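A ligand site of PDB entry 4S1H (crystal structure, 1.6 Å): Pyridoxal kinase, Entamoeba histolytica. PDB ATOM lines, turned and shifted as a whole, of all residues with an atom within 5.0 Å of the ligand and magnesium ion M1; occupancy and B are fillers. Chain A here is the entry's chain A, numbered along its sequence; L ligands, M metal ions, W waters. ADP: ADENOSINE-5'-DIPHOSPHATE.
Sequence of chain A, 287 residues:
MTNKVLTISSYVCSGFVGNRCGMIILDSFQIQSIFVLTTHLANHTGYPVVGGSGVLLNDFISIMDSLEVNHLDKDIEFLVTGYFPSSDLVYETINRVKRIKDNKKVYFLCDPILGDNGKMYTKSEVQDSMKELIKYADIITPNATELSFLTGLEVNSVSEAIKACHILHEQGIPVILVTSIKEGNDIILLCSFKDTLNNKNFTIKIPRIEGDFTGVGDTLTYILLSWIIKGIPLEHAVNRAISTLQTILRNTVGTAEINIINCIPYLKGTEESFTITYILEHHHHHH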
ATOM      1  N   ASP A 116       5.296  -6.898  21.848  1.00  0.00           N
ATOM      2  CA  ASP A 116       3.844  -6.904  21.909  1.00  0.00           C
ATOM      3  C   ASP A 116       3.389  -8.231  22.496  1.00  0.00           C
ATOM      4  O   ASP A 116       4.161  -9.204  22.528  1.00  0.00           O
ATOM      5  CB  ASP A 116       3.254  -6.719  20.503  1.00  0.00           C
ATOM      6  CG  ASP A 116       1.860  -6.102  20.518  1.00  0.00           C
ATOM      7  OD1 ASP A 116       1.261  -5.967  21.611  1.00  0.00           O
ATOM      8  OD2 ASP A 116       1.385  -5.718  19.416  1.00  0.00           O
ATOM      9  N   ASN A 143       2.776   0.655  23.117  1.00  0.00           N
ATOM     10  CA  ASN A 143       1.685  -0.231  23.489  1.00  0.00           C
ATOM     11  C   ASN A 143       1.836  -0.662  24.967  1.00  0.00           C
ATOM     12  O   ASN A 143       2.808  -0.308  25.651  1.00  0.00           O
ATOM     13  CB  ASN A 143       1.554  -1.422  22.512  1.00  0.00           C
ATOM     14  CG  ASN A 143       2.741  -2.365  22.567  1.00  0.00           C
ATOM     15  OD1 ASN A 143       3.415  -2.486  23.587  1.00  0.00           O
ATOM     16  ND2 ASN A 143       3.016  -3.035  21.440  1.00  0.00           N
ATOM     17  N   GLU A 146       5.112  -2.556  25.812  1.00  0.00           N
ATOM     18  CA  GLU A 146       6.257  -1.672  25.781  1.00  0.00           C
ATOM     19  C   GLU A 146       6.298  -0.816  27.047  1.00  0.00           C
ATOM     20  O   GLU A 146       7.370  -0.691  27.660  1.00  0.00           O
ATOM     21  CB  GLU A 146       6.302  -0.860  24.494  1.00  0.00           C
ATOM     22  CG  GLU A 146       6.588  -1.779  23.330  1.00  0.00           C
ATOM     23  CD  GLU A 146       6.132  -1.292  21.995  1.00  0.00           C
ATOM     24  OE1 GLU A 146       5.265  -0.377  21.937  1.00  0.00           O
ATOM     25  OE2 GLU A 146       6.690  -1.841  20.996  1.00  0.00           O
ATOM     26  N   THR A 179      -1.037   2.987  23.427  1.00  0.00           N
ATOM     27  CA  THR A 179      -1.773   2.845  22.141  1.00  0.00           C
ATOM     28  C   THR A 179      -2.729   1.667  22.166  1.00  0.00           C
ATOM     29  O   THR A 179      -3.633   1.582  21.332  1.00  0.00           O
ATOM     30  CB  THR A 179      -0.826   2.727  20.934  1.00  0.00           C
ATOM     31  OG1 THR A 179       0.073   1.618  21.060  1.00  0.00           O
ATOM     32  CG2 THR A 179       0.002   3.985  20.786  1.00  0.00           C
ATOM     33  N   SER A 180      -2.474   0.701  23.050  1.00  0.00           N
ATOM     34  CA  SER A 180      -3.335  -0.458  23.157  1.00  0.00           C
ATOM     35  C   SER A 180      -3.199  -1.115  24.492  1.00  0.00           C
ATOM     36  O   SER A 180      -2.096  -1.456  24.920  1.00  0.00           O
ATOM     37  CB  SER A 180      -3.080  -1.503  22.055  1.00  0.00           C
ATOM     38  OG  SER A 180      -1.744  -1.942  21.988  1.00  0.00           O
ATOM     39  N   ILE A 187      -9.917  -2.676  22.540  1.00  0.00           N
ATOM     40  CA  ILE A 187      -8.608  -2.112  22.778  1.00  0.00           C
ATOM     41  C   ILE A 187      -8.888  -0.760  23.396  1.00  0.00           C
ATOM     42  O   ILE A 187      -9.601   0.069  22.812  1.00  0.00           O
ATOM     43  CB  ILE A 187      -7.895  -1.956  21.393  1.00  0.00           C
ATOM     44  CG1 ILE A 187      -7.558  -3.345  20.824  1.00  0.00           C
ATOM     45  CG2 ILE A 187      -6.639  -1.081  21.510  1.00  0.00           C
ATOM     46  CD1 ILE A 187      -7.077  -3.293  19.384  1.00  0.00           C
ATOM     47  N   LEU A 189      -7.133   2.844  24.394  1.00  0.00           N
ATOM     48  CA  LEU A 189      -6.036   3.759  24.305  1.00  0.00           C
ATOM     49  C   LEU A 189      -6.149   4.712  25.476  1.00  0.00           C
ATOM     50  O   LEU A 189      -7.243   5.136  25.804  1.00  0.00           O
ATOM     51  CB  LEU A 189      -6.091   4.489  22.961  1.00  0.00           C
ATOM     52  CG  LEU A 189      -5.174   5.675  22.716  1.00  0.00           C
ATOM     53  CD1 LEU A 189      -4.726   5.686  21.238  1.00  0.00           C
ATOM     54  CD2 LEU A 189      -5.832   6.982  23.097  1.00  0.00           C
ATOM     55  N   ILE A 206     -11.808   1.112  21.362  1.00  0.00           N
ATOM     56  CA  ILE A 206     -11.742   0.689  19.958  1.00  0.00           C
ATOM     57  C   ILE A 206     -12.140  -0.789  19.854  1.00  0.00           C
ATOM     58  O   ILE A 206     -11.501  -1.618  20.473  1.00  0.00           O
ATOM     59  CB  ILE A 206     -10.316   0.849  19.433  1.00  0.00           C
ATOM     60  CG1 ILE A 206      -9.875   2.317  19.563  1.00  0.00           C
ATOM     61  CG2 ILE A 206     -10.213   0.368  17.981  1.00  0.00           C
ATOM     62  CD1 ILE A 206      -8.408   2.494  19.868  1.00  0.00           C
ATOM     63  N   PRO A 207     -13.155  -1.117  19.023  1.00  0.00           N
ATOM     64  CA  PRO A 207     -13.509  -2.545  18.885  1.00  0.00           C
ATOM     65  C   PRO A 207     -12.408  -3.290  18.191  1.00  0.00           C
ATOM     66  O   PRO A 207     -11.874  -2.754  17.205  1.00  0.00           O
ATOM     67  CB  PRO A 207     -14.768  -2.528  18.018  1.00  0.00           C
ATOM     68  CG  PRO A 207     -15.344  -1.163  18.190  1.00  0.00           C
ATOM     69  CD  PRO A 207     -14.153  -0.248  18.371  1.00  0.00           C
ATOM     70  N   ARG A 208     -12.021  -4.455  18.687  1.00  0.00           N
ATOM     71  CA  ARG A 208     -10.941  -5.203  18.051  1.00  0.00           C
ATOM     72  C   ARG A 208     -11.420  -5.784  16.721  1.00  0.00           C
ATOM     73  O   ARG A 208     -12.517  -6.343  16.646  1.00  0.00           O
ATOM     74  CB  ARG A 208     -10.431  -6.343  18.939  1.00  0.00           C
ATOM     75  CG  ARG A 208      -9.116  -6.930  18.409  1.00  0.00           C
ATOM     76  CD  ARG A 208      -8.696  -8.167  19.216  1.00  0.00           C
ATOM     77  NE  ARG A 208      -7.994  -7.845  20.452  1.00  0.00           N
ATOM     78  CZ  ARG A 208      -6.785  -7.289  20.519  1.00  0.00           C
ATOM     79  NH1 ARG A 208      -6.116  -6.971  19.414  1.00  0.00           N
ATOM     80  NH2 ARG A 208      -6.241  -7.049  21.706  1.00  0.00           N
ATOM     81  N   ILE A 209     -10.606  -5.639  15.695  1.00  0.00           N
ATOM     82  CA  ILE A 209     -10.810  -6.289  14.409  1.00  0.00           C
ATOM     83  C   ILE A 209      -9.945  -7.545  14.453  1.00  0.00           C
ATOM     84  O   ILE A 209      -8.798  -7.484  14.875  1.00  0.00           O
ATOM     85  CB  ILE A 209     -10.367  -5.369  13.250  1.00  0.00           C
ATOM     86  CG1 ILE A 209     -11.244  -4.109  13.202  1.00  0.00           C
ATOM     87  CG2 ILE A 209     -10.392  -6.131  11.929  1.00  0.00           C
ATOM     88  CD1 ILE A 209     -10.747  -3.023  12.265  1.00  0.00           C
ATOM     89  N   GLY A 211      -7.387 -10.386  13.955  1.00  0.00           N
ATOM     90  CA  GLY A 211      -6.042 -10.391  13.379  1.00  0.00           C
ATOM     91  C   GLY A 211      -5.047  -9.715  14.295  1.00  0.00           C
ATOM     92  O   GLY A 211      -5.419  -8.786  15.038  1.00  0.00           O
ATOM     93  N   ASP A 212      -3.786 -10.153  14.241  1.00  0.00           N
ATOM     94  CA  ASP A 212      -2.659  -9.348  14.779  1.00  0.00           C
ATOM     95  C   ASP A 212      -1.921  -8.750  13.574  1.00  0.00           C
ATOM     96  O   ASP A 212      -1.388  -9.472  12.715  1.00  0.00           O
ATOM     97  CB  ASP A 212      -1.694 -10.085  15.741  1.00  0.00           C
ATOM     98  CG  ASP A 212      -0.991  -9.122  16.730  1.00  0.00           C
ATOM     99  OD1 ASP A 212      -1.673  -8.490  17.575  1.00  0.00           O
ATOM    100  OD2 ASP A 212       0.247  -8.988  16.682  1.00  0.00           O
ATOM    101  N   PHE A 213      -1.917  -7.424  13.526  1.00  0.00           N
ATOM    102  CA  PHE A 213      -1.437  -6.680  12.365  1.00  0.00           C
ATOM    103  C   PHE A 213      -0.039  -6.170  12.660  1.00  0.00           C
ATOM    104  O   PHE A 213       0.331  -5.953  13.830  1.00  0.00           O
ATOM    105  CB  PHE A 213      -2.385  -5.512  12.052  1.00  0.00           C
ATOM    106  CG  PHE A 213      -3.766  -5.947  11.617  1.00  0.00           C
ATOM    107  CD1 PHE A 213      -3.996  -6.343  10.283  1.00  0.00           C
ATOM    108  CD2 PHE A 213      -4.819  -6.000  12.521  1.00  0.00           C
ATOM    109  CE1 PHE A 213      -5.241  -6.744   9.873  1.00  0.00           C
ATOM    110  CE2 PHE A 213      -6.076  -6.409  12.114  1.00  0.00           C
ATOM    111  CZ  PHE A 213      -6.291  -6.795  10.790  1.00  0.00           C
ATOM    112  N   GLY A 215       2.922  -3.235  11.660  1.00  0.00           N
ATOM    113  CA  GLY A 215       3.015  -1.828  11.222  1.00  0.00           C
ATOM    114  C   GLY A 215       1.901  -0.893  11.651  1.00  0.00           C
ATOM    115  O   GLY A 215       1.859   0.279  11.229  1.00  0.00           O
ATOM    116  N   VAL A 216       0.983  -1.364  12.475  1.00  0.00           N
ATOM    117  CA  VAL A 216      -0.155  -0.524  12.864  1.00  0.00           C
ATOM    118  C   VAL A 216       0.229   0.586  13.826  1.00  0.00           C
ATOM    119  O   VAL A 216      -0.201   1.735  13.691  1.00  0.00           O
ATOM    120  CB  VAL A 216      -1.343  -1.348  13.417  1.00  0.00           C
ATOM    121  CG1 VAL A 216      -2.116  -1.962  12.276  1.00  0.00           C
ATOM    122  CG2 VAL A 216      -0.915  -2.435  14.410  1.00  0.00           C
ATOM    123  N   GLY A 217       1.055   0.268  14.808  1.00  0.00           N
ATOM    124  CA  GLY A 217       1.585   1.271  15.699  1.00  0.00           C
ATOM    125  C   GLY A 217       2.411   2.302  14.982  1.00  0.00           C
ATOM    126  O   GLY A 217       2.363   3.478  15.308  1.00  0.00           O
ATOM    127  N   ASP A 218       3.221   1.846  14.020  1.00  0.00           N
ATOM    128  CA  ASP A 218       4.006   2.785  13.223  1.00  0.00           C
ATOM    129  C   ASP A 218       3.098   3.738  12.432  1.00  0.00           C
ATOM    130  O   ASP A 218       3.347   4.944  12.376  1.00  0.00           O
ATOM    131  CB  ASP A 218       4.940   1.994  12.270  1.00  0.00           C
ATOM    132  CG  ASP A 218       5.857   1.001  13.019  1.00  0.00           C
ATOM    133  OD1 ASP A 218       6.133   1.241  14.235  1.00  0.00           O
ATOM    134  OD2 ASP A 218       6.299  -0.007  12.408  1.00  0.00           O
ATOM    135  N   LEU A 220      -0.011   4.552  13.101  1.00  0.00           N
ATOM    136  CA  LEU A 220      -0.579   5.506  14.072  1.00  0.00           C
ATOM    137  C   LEU A 220       0.366   6.677  14.369  1.00  0.00           C
ATOM    138  O   LEU A 220      -0.049   7.854  14.352  1.00  0.00           O
ATOM    139  CB  LEU A 220      -0.974   4.819  15.402  1.00  0.00           C
ATOM    140  CG  LEU A 220      -1.452   5.727  16.568  1.00  0.00           C
ATOM    141  CD1 LEU A 220      -2.647   6.573  16.174  1.00  0.00           C
ATOM    142  CD2 LEU A 220      -1.753   4.891  17.780  1.00  0.00           C
ATOM    143  N   ILE A 242      -6.630   7.421  14.891  1.00  0.00           N
ATOM    144  CA  ILE A 242      -7.239   6.138  15.219  1.00  0.00           C
ATOM    145  C   ILE A 242      -8.376   5.822  14.258  1.00  0.00           C
ATOM    146  O   ILE A 242      -8.549   4.678  13.856  1.00  0.00           O
ATOM    147  CB  ILE A 242      -7.753   6.157  16.688  1.00  0.00           C
ATOM    148  CG1 ILE A 242      -6.538   6.287  17.616  1.00  0.00           C
ATOM    149  CG2 ILE A 242      -8.686   4.970  17.004  1.00  0.00           C
ATOM    150  CD1 ILE A 242      -5.762   5.050  17.933  1.00  0.00           C
ATOM    151  N   LEU A 245      -6.883   4.802  10.941  1.00  0.00           N
ATOM    152  CA  LEU A 245      -6.372   3.433  11.090  1.00  0.00           C
ATOM    153  C   LEU A 245      -7.462   2.375  11.047  1.00  0.00           C
ATOM    154  O   LEU A 245      -7.275   1.305  10.441  1.00  0.00           O
ATOM    155  CB  LEU A 245      -5.560   3.328  12.380  1.00  0.00           C
ATOM    156  CG  LEU A 245      -4.527   2.216  12.588  1.00  0.00           C
ATOM    157  CD1 LEU A 245      -3.759   1.791  11.345  1.00  0.00           C
ATOM    158  CD2 LEU A 245      -3.546   2.690  13.653  1.00  0.00           C
ATOM    159  N   GLN A 246      -8.624   2.630  11.667  1.00  0.00           N
ATOM    160  CA  GLN A 246      -9.743   1.685  11.566  1.00  0.00           C
ATOM    161  C   GLN A 246     -10.158   1.486  10.132  1.00  0.00           C
ATOM    162  O   GLN A 246     -10.383   0.371   9.682  1.00  0.00           O
ATOM    163  CB  GLN A 246     -10.968   2.117  12.395  1.00  0.00           C
ATOM    164  CG  GLN A 246     -10.851   1.864  13.867  1.00  0.00           C
ATOM    165  CD  GLN A 246     -10.631   0.393  14.219  1.00  0.00           C
ATOM    166  OE1 GLN A 246      -9.527  -0.068  14.441  1.00  0.00           O
ATOM    167  NE2 GLN A 246     -11.721  -0.363  14.234  1.00  0.00           N
ATOM    168  N   LEU A 249      -7.570  -0.778   8.450  1.00  0.00           N
ATOM    169  CA  LEU A 249      -7.696  -2.181   8.875  1.00  0.00           C
ATOM    170  C   LEU A 249      -8.952  -2.878   8.358  1.00  0.00           C
ATOM    171  O   LEU A 249      -8.905  -4.040   7.957  1.00  0.00           O
ATOM    172  CB  LEU A 249      -7.645  -2.277  10.389  1.00  0.00           C
ATOM    173  CG  LEU A 249      -6.300  -1.866  10.926  1.00  0.00           C
ATOM    174  CD1 LEU A 249      -6.366  -1.914  12.414  1.00  0.00           C
ATOM    175  CD2 LEU A 249      -5.181  -2.772  10.440  1.00  0.00           C
HETATM  176  PB  ADP L   1       1.794  -1.705  17.937  1.00  0.00           P
HETATM  177  O1B ADP L   1       1.477  -2.934  18.761  1.00  0.00           O
HETATM  178  O2B ADP L   1       2.112  -2.032  16.480  1.00  0.00           O
HETATM  179  O3B ADP L   1       2.746  -0.802  18.643  1.00  0.00           O
HETATM  180  PA  ADP L   1      -0.986  -1.156  18.557  1.00  0.00           P
HETATM  181  O1A ADP L   1      -1.039  -0.429  19.867  1.00  0.00           O
HETATM  182  O2A ADP L   1      -1.224  -2.635  18.535  1.00  0.00           O
HETATM  183  O3A ADP L   1       0.435  -0.864  17.832  1.00  0.00           O
HETATM  184  O5' ADP L   1      -1.982  -0.494  17.526  1.00  0.00           O
HETATM  185  C5' ADP L   1      -1.985   0.885  17.206  1.00  0.00           C
HETATM  186  C4' ADP L   1      -3.407   1.262  16.898  1.00  0.00           C
HETATM  187  O4' ADP L   1      -3.881   0.452  15.819  1.00  0.00           O
HETATM  188  C3' ADP L   1      -4.331   0.962  18.079  1.00  0.00           C
HETATM  189  O3' ADP L   1      -4.441   2.092  18.953  1.00  0.00           O
HETATM  190  C2' ADP L   1      -5.620   0.614  17.393  1.00  0.00           C
HETATM  191  O2' ADP L   1      -6.332   1.798  17.065  1.00  0.00           O
HETATM  192  C1' ADP L   1      -5.188  -0.047  16.089  1.00  0.00           C
HETATM  193  N9  ADP L   1      -5.176  -1.527  16.109  1.00  0.00           N
HETATM  194  C8  ADP L   1      -4.133  -2.372  16.198  1.00  0.00           C
HETATM  195  N7  ADP L   1      -4.538  -3.669  16.146  1.00  0.00           N
HETATM  196  C5  ADP L   1      -5.868  -3.652  16.007  1.00  0.00           C
HETATM  197  C6  ADP L   1      -6.941  -4.661  15.873  1.00  0.00           C
HETATM  198  N6  ADP L   1      -6.621  -5.977  15.897  1.00  0.00           N
HETATM  199  N1  ADP L   1      -8.209  -4.220  15.743  1.00  0.00           N
HETATM  200  C2  ADP L   1      -8.519  -2.887  15.729  1.00  0.00           C
HETATM  201  N3  ADP L   1      -7.585  -1.914  15.847  1.00  0.00           N
HETATM  202  C4  ADP L   1      -6.279  -2.238  15.973  1.00  0.00           C
HETATM  203 MG    MG M   1      -0.122  -4.213  18.858  1.00  0.00          MG
HETATM  204 MG    MG M   2       4.052   2.811  19.298  1.00  0.00          MG
HETATM  205  O   HOH W   1       4.843  -0.640  16.100  1.00  0.00           O
HETATM  206  O   HOH W   2      -3.876  -3.273  19.497  1.00  0.00           O
HETATM  207  O   HOH W   3       5.330  -1.857  18.690  1.00  0.00           O
HETATM  208  O   HOH W   4       4.336   1.815  17.339  1.00  0.00           O
HETATM  209  O   HOH W   5      -2.772  -6.072  16.113  1.00  0.00           O
HETATM  210  O   HOH W   6      -0.512  -3.950  20.854  1.00  0.00           O
HETATM  211  O   HOH W   7       3.804  -4.198  18.019  1.00  0.00           O
HETATM  212  O   HOH W   8       2.364   1.692  19.643  1.00  0.00           O
HETATM  213  O   HOH W   9       0.278  -4.501  16.746  1.00  0.00           O
HETATM  214  O   HOH W  10      -7.946   2.167  15.082  1.00  0.00           O
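Magnesium ion M1 is bound by an oxygen (O2A) of the ligand, an oxygen (O1B) of the ligand, water W6, water W9 and the side-chain carboxylate of Asp 116.
OD1 of Asp 116 lies close to ND2 of Asn 143 (3.4 Å). N of Glu 146 is in hydrogen-bond range of OD1 of Asn 143, at 2.8 Å. The backbone carbonyl oxygen of Ile 206 is in hydrogen-bond range of the backbone NH of Ile 187, at 2.8 Å.
A nitrogen (N3) of the ligand sits close to the side-chain amide oxygen (OE1) of Gln 246 (3.0 Å). A nitrogen (N6) of the ligand is in hydrogen-bond range of the backbone carbonyl oxygen (O) of Gly 211, at 3.2 Å. O3' of the ligand is in hydrogen-bond range of O of Thr 179 (2.6 Å). O1B of the ligand sits close to ND2 of Asn 143 (3.1 Å). An oxygen (O2B) of the ligand is in hydrogen-bond range of the backbone NH of Gly 217 (3.0 Å). The side-chain hydroxyl (OG1) of Thr 179 is in hydrogen-bond range of an oxygen (O1A) of the ligand, 2.6 Å away. A nitrogen (N6) of the ligand sits at hydrogen-bond distance from the backbone carbonyl oxygen (O) of Ile 209, 2.8 Å away. N of Ile 209 is in hydrogen-bond range of N1 of the ligand, 2.8 Å away. OG of Ser 180 is in hydrogen-bond range of O1A of the ligand.
Water W9 lies within hydrogen-bond range of O2B of the ligand (3.1 Å) and O of Phe 213 (3.3 Å). Water W10 lies within hydrogen-bond range of an oxygen (O2') of the ligand (2.6 Å), the side-chain amide oxygen (OE1) of Gln 246 (2.8 Å) and the backbone carbonyl oxygen (O) of Ile 242 (2.9 Å). Water W8 lies within hydrogen-bond range of OG1 of Thr 179 and O3B of the ligand. Water W3 lies within hydrogen-bond range of the side-chain carboxylate of Glu 146 (2.7 Å) and an oxygen (O3B) of the ligand (2.8 Å). Water W1 lies within hydrogen-bond range of the side-chain carboxylate of Asp 218 and an oxygen (O2B) of the ligand. Water W4 lies within hydrogen-bond range of the backbone carbonyl oxygen of Gly 217 (3.3 Å) and an oxygen (O3B) of the ligand (3.3 Å).
CD1 of Ile 187 touches C5 of the ligand, at 3.6 Å. Ile 206 touches the ligand. O of Pro 207 touches C2 of the ligand, at 3.7 Å. CG of Arg 208 touches N6 of the ligand, 3.7 Å away. Phe 213 touches the ligand. CG2 of Val 216 touches C8 of the ligand (3.7 Å). Ile 242 touches the ligand (CD1 to O3', 3.4 Å). CD2 of Leu 245 touches O4' of the ligand, at 3.1 Å. CD1 of Leu 249 touches C4 of the ligand, 3.6 Å away. Hydrophobic or aromatic side chains within 4 Å of the ligand: Ile 187, Ile 206, Ile 209, Phe 213, Val 216, Ile 242, Leu 245 and Leu 249. Within 4 Å of the ligand: Asp 116, Asn 143, Thr 179, Ser 180, Ile 187, Ile 206, Pro 207, Arg 208, Ile 209, Gly 211, Phe 213, Val 216, Gly 217, Ile 242, Leu 245, Gln 246 and Leu 249.
Within 4 Å of magnesium ion M1: Asp 116. The nearest printed residue that does not touch magnesium ion M1 is Ser 180 (4.2 Å).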
